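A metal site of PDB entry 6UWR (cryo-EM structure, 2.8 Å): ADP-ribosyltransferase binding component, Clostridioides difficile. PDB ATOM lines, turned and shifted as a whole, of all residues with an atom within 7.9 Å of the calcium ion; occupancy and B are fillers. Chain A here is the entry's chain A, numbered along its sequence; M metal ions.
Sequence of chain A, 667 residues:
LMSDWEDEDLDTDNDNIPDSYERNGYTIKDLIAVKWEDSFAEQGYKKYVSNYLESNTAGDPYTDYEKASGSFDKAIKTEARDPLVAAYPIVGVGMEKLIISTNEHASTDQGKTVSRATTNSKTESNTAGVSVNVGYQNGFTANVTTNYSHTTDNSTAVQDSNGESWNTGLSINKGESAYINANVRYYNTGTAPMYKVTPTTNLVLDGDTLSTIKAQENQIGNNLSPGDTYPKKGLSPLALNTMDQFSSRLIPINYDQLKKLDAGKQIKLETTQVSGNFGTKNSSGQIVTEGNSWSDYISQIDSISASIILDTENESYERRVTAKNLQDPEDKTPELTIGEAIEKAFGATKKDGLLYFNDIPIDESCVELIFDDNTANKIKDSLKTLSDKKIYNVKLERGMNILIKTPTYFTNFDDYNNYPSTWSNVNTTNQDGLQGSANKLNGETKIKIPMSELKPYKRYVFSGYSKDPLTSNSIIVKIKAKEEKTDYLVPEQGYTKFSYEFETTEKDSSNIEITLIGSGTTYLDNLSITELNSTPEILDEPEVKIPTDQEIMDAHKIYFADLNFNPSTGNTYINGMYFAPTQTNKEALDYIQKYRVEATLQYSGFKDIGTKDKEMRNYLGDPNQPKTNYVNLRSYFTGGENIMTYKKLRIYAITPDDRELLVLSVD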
ATOM      1  N   PHE A 410      -6.820 -38.257  14.002  1.00  0.00           N
ATOM      2  CA  PHE A 410      -5.722 -37.307  14.011  1.00  0.00           C
ATOM      3  C   PHE A 410      -6.131 -36.073  13.230  1.00  0.00           C
ATOM      4  O   PHE A 410      -6.862 -36.166  12.253  1.00  0.00           O
ATOM      5  CB  PHE A 410      -4.462 -37.931  13.409  1.00  0.00           C
ATOM      6  CG  PHE A 410      -3.299 -36.998  13.307  1.00  0.00           C
ATOM      7  CD1 PHE A 410      -2.543 -36.704  14.417  1.00  0.00           C
ATOM      8  CD2 PHE A 410      -2.949 -36.437  12.104  1.00  0.00           C
ATOM      9  CE1 PHE A 410      -1.466 -35.846  14.325  1.00  0.00           C
ATOM     10  CE2 PHE A 410      -1.886 -35.582  12.012  1.00  0.00           C
ATOM     11  CZ  PHE A 410      -1.143 -35.291  13.121  1.00  0.00           C
ATOM     12  N   THR A 411      -5.649 -34.915  13.682  1.00  0.00           N
ATOM     13  CA  THR A 411      -5.800 -33.672  12.925  1.00  0.00           C
ATOM     14  C   THR A 411      -4.574 -32.809  13.139  1.00  0.00           C
ATOM     15  O   THR A 411      -4.033 -32.725  14.253  1.00  0.00           O
ATOM     16  CB  THR A 411      -7.068 -32.915  13.330  1.00  0.00           C
ATOM     17  OG1 THR A 411      -7.247 -31.792  12.450  1.00  0.00           O
ATOM     18  CG2 THR A 411      -6.987 -32.421  14.757  1.00  0.00           C
ATOM     19  N   ASN A 412      -4.103 -32.185  12.062  1.00  0.00           N
ATOM     20  CA  ASN A 412      -3.065 -31.172  12.135  1.00  0.00           C
ATOM     21  C   ASN A 412      -3.613 -29.774  11.909  1.00  0.00           C
ATOM     22  O   ASN A 412      -2.853 -28.807  11.963  1.00  0.00           O
ATOM     23  CB  ASN A 412      -1.977 -31.470  11.104  1.00  0.00           C
ATOM     24  CG  ASN A 412      -2.538 -31.903   9.785  1.00  0.00           C
ATOM     25  OD1 ASN A 412      -3.756 -32.074   9.656  1.00  0.00           O
ATOM     26  ND2 ASN A 412      -1.689 -32.074   8.792  1.00  0.00           N
ATOM     27  N   PHE A 413      -4.916 -29.666  11.644  1.00  0.00           N
ATOM     28  CA  PHE A 413      -5.618 -28.419  11.379  1.00  0.00           C
ATOM     29  C   PHE A 413      -5.186 -27.754  10.071  1.00  0.00           C
ATOM     30  O   PHE A 413      -5.535 -26.604   9.825  1.00  0.00           O
ATOM     31  CB  PHE A 413      -5.478 -27.423  12.539  1.00  0.00           C
ATOM     32  CG  PHE A 413      -5.810 -27.989  13.880  1.00  0.00           C
ATOM     33  CD1 PHE A 413      -7.093 -28.361  14.189  1.00  0.00           C
ATOM     34  CD2 PHE A 413      -4.829 -28.114  14.844  1.00  0.00           C
ATOM     35  CE1 PHE A 413      -7.403 -28.879  15.425  1.00  0.00           C
ATOM     36  CE2 PHE A 413      -5.139 -28.632  16.080  1.00  0.00           C
ATOM     37  CZ  PHE A 413      -6.420 -29.009  16.372  1.00  0.00           C
ATOM     38  N   ASP A 414      -4.437 -28.453   9.228  1.00  0.00           N
ATOM     39  CA  ASP A 414      -4.110 -27.935   7.902  1.00  0.00           C
ATOM     40  C   ASP A 414      -4.760 -28.754   6.804  1.00  0.00           C
ATOM     41  O   ASP A 414      -5.552 -28.225   6.020  1.00  0.00           O
ATOM     42  CB  ASP A 414      -2.596 -27.938   7.660  1.00  0.00           C
ATOM     43  CG  ASP A 414      -1.810 -27.562   8.874  1.00  0.00           C
ATOM     44  OD1 ASP A 414      -2.400 -27.119   9.865  1.00  0.00           O
ATOM     45  OD2 ASP A 414      -0.580 -27.759   8.849  1.00  0.00           O
ATOM     46  N   ASP A 415      -4.459 -30.043   6.731  1.00  0.00           N
ATOM     47  CA  ASP A 415      -4.751 -30.868   5.567  1.00  0.00           C
ATOM     48  C   ASP A 415      -5.355 -32.210   5.914  1.00  0.00           C
ATOM     49  O   ASP A 415      -5.969 -32.830   5.036  1.00  0.00           O
ATOM     50  CB  ASP A 415      -3.474 -31.102   4.748  1.00  0.00           C
ATOM     51  CG  ASP A 415      -3.709 -31.006   3.265  1.00  0.00           C
ATOM     52  OD1 ASP A 415      -2.856 -30.431   2.566  1.00  0.00           O
ATOM     53  OD2 ASP A 415      -4.757 -31.516   2.795  1.00  0.00           O
ATOM     54  N   ASP A 432       1.324 -20.915  13.042  1.00  0.00           N
ATOM     55  CA  ASP A 432       1.886 -21.450  14.275  1.00  0.00           C
ATOM     56  C   ASP A 432       1.583 -22.940  14.347  1.00  0.00           C
ATOM     57  O   ASP A 432       1.138 -23.560  13.381  1.00  0.00           O
ATOM     58  CB  ASP A 432       1.358 -20.685  15.485  1.00  0.00           C
ATOM     59  CG  ASP A 432       2.089 -19.375  15.692  1.00  0.00           C
ATOM     60  OD1 ASP A 432       3.328 -19.358  15.531  1.00  0.00           O
ATOM     61  OD2 ASP A 432       1.427 -18.364  16.027  1.00  0.00           O
ATOM     62  N   GLY A 433       1.857 -23.536  15.497  1.00  0.00           N
ATOM     63  CA  GLY A 433       1.839 -24.977  15.581  1.00  0.00           C
ATOM     64  C   GLY A 433       3.068 -25.546  14.915  1.00  0.00           C
ATOM     65  O   GLY A 433       3.776 -24.862  14.172  1.00  0.00           O
ATOM     66  N   LEU A 434       3.339 -26.812  15.204  1.00  0.00           N
ATOM     67  CA  LEU A 434       4.491 -27.469  14.596  1.00  0.00           C
ATOM     68  C   LEU A 434       4.502 -27.266  13.085  1.00  0.00           C
ATOM     69  O   LEU A 434       5.573 -27.081  12.492  1.00  0.00           O
ATOM     70  CB  LEU A 434       4.478 -28.963  14.930  1.00  0.00           C
ATOM     71  CG  LEU A 434       4.728 -29.296  16.395  1.00  0.00           C
ATOM     72  CD1 LEU A 434       4.107 -30.624  16.717  1.00  0.00           C
ATOM     73  CD2 LEU A 434       6.215 -29.319  16.693  1.00  0.00           C
ATOM     74  N   GLN A 435       3.327 -27.269  12.466  1.00  0.00           N
ATOM     75  CA  GLN A 435       3.174 -26.958  11.043  1.00  0.00           C
ATOM     76  C   GLN A 435       1.845 -26.209  10.865  1.00  0.00           C
ATOM     77  O   GLN A 435       0.778 -26.821  10.822  1.00  0.00           O
ATOM     78  CB  GLN A 435       3.226 -28.219  10.197  1.00  0.00           C
ATOM     79  CG  GLN A 435       4.489 -29.068  10.377  1.00  0.00           C
ATOM     80  CD  GLN A 435       4.213 -30.377  11.106  1.00  0.00           C
ATOM     81  OE1 GLN A 435       3.164 -30.992  10.944  1.00  0.00           O
ATOM     82  NE2 GLN A 435       5.172 -30.811  11.913  1.00  0.00           N
ATOM     83  N   GLY A 436       1.921 -24.873  10.814  1.00  0.00           N
ATOM     84  CA  GLY A 436       0.848 -23.997  10.370  1.00  0.00           C
ATOM     85  C   GLY A 436      -0.549 -24.111  10.943  1.00  0.00           C
ATOM     86  O   GLY A 436      -1.511 -24.103  10.166  1.00  0.00           O
ATOM     87  N   SER A 437      -0.709 -24.161  12.261  1.00  0.00           N
ATOM     88  CA  SER A 437      -2.036 -24.364  12.828  1.00  0.00           C
ATOM     89  C   SER A 437      -2.063 -24.048  14.309  1.00  0.00           C
ATOM     90  O   SER A 437      -1.076 -24.265  15.016  1.00  0.00           O
ATOM     91  CB  SER A 437      -2.503 -25.793  12.613  1.00  0.00           C
ATOM     92  OG  SER A 437      -1.406 -26.639  12.305  1.00  0.00           O
ATOM     93  N   ALA A 438      -3.194 -23.538  14.784  1.00  0.00           N
ATOM     94  CA  ALA A 438      -3.361 -23.237  16.206  1.00  0.00           C
ATOM     95  C   ALA A 438      -4.556 -23.961  16.828  1.00  0.00           C
ATOM     96  O   ALA A 438      -4.391 -24.664  17.825  1.00  0.00           O
ATOM     97  CB  ALA A 438      -3.512 -21.726  16.399  1.00  0.00           C
ATOM     98  N   LEU A 524      -2.306 -25.150  19.996  1.00  0.00           N
ATOM     99  CA  LEU A 524      -2.365 -26.610  19.935  1.00  0.00           C
ATOM    100  C   LEU A 524      -2.097 -27.080  18.512  1.00  0.00           C
ATOM    101  O   LEU A 524      -2.367 -26.359  17.553  1.00  0.00           O
ATOM    102  CB  LEU A 524      -3.736 -27.128  20.381  1.00  0.00           C
ATOM    103  CG  LEU A 524      -4.257 -26.757  21.769  1.00  0.00           C
ATOM    104  CD1 LEU A 524      -5.627 -27.348  21.963  1.00  0.00           C
ATOM    105  CD2 LEU A 524      -3.317 -27.245  22.848  1.00  0.00           C
ATOM    106  N   ASP A 525      -1.564 -28.293  18.394  1.00  0.00           N
ATOM    107  CA  ASP A 525      -1.352 -28.883  17.077  1.00  0.00           C
ATOM    108  C   ASP A 525      -1.221 -30.383  17.220  1.00  0.00           C
ATOM    109  O   ASP A 525      -0.797 -30.892  18.266  1.00  0.00           O
ATOM    110  CB  ASP A 525      -0.102 -28.308  16.387  1.00  0.00           C
ATOM    111  CG  ASP A 525      -0.282 -28.132  14.896  1.00  0.00           C
ATOM    112  OD1 ASP A 525      -1.421 -28.250  14.404  1.00  0.00           O
ATOM    113  OD2 ASP A 525       0.720 -27.880  14.207  1.00  0.00           O
ATOM    114  N   ASN A 526      -1.612 -31.103  16.165  1.00  0.00           N
ATOM    115  CA  ASN A 526      -1.415 -32.539  16.044  1.00  0.00           C
ATOM    116  C   ASN A 526      -2.082 -33.301  17.184  1.00  0.00           C
ATOM    117  O   ASN A 526      -1.435 -33.966  17.991  1.00  0.00           O
ATOM    118  CB  ASN A 526       0.083 -32.862  15.966  1.00  0.00           C
ATOM    119  CG  ASN A 526       0.746 -32.242  14.763  1.00  0.00           C
ATOM    120  OD1 ASN A 526       1.944 -31.956  14.779  1.00  0.00           O
ATOM    121  ND2 ASN A 526      -0.015 -32.052  13.708  1.00  0.00           N
ATOM    122  N   LEU A 527      -3.411 -33.219  17.229  1.00  0.00           N
ATOM    123  CA  LEU A 527      -4.181 -33.888  18.267  1.00  0.00           C
ATOM    124  C   LEU A 527      -4.629 -35.267  17.793  1.00  0.00           C
ATOM    125  O   LEU A 527      -5.244 -35.385  16.738  1.00  0.00           O
ATOM    126  CB  LEU A 527      -5.376 -33.036  18.661  1.00  0.00           C
ATOM    127  CG  LEU A 527      -5.054 -31.753  19.427  1.00  0.00           C
ATOM    128  CD1 LEU A 527      -6.210 -30.815  19.388  1.00  0.00           C
ATOM    129  CD2 LEU A 527      -4.703 -32.076  20.862  1.00  0.00           C
HETATM  130 CA    CA M   1      -0.234 -28.535  12.201  1.00  0.00          CA
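OD2 of Asp 414 touches the calcium ion, 3.5 Å away. Asn 526 touches the calcium ion (ND2 to CA, 3.8 Å). The nearest printed residue that does not touch the calcium ion is Gly 436 (4.5 Å).
OG of Ser 437 sits close to OD1 of Asp 414 (2.7 Å). The backbone NH of Leu 434 lies close to the side-chain carboxylate of Asp 525 (3.0 Å). O of Gln 435 lies close to OD2 of Asp 414. The backbone carbonyl oxygen of Asn 412 lies close to the side-chain carboxylate of Asp 414, at 2.7 Å. N of Asn 526 lies close to O of Thr 411 (3.5 Å).
The calcium ion is bound by OG of Ser 437 (2.2 Å), OD2 of Asp 525 (2.3 Å), O of Gln 435 (2.4 Å), OD1 of Asp 525 (2.5 Å) and O of Asn 412 (2.6 Å).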
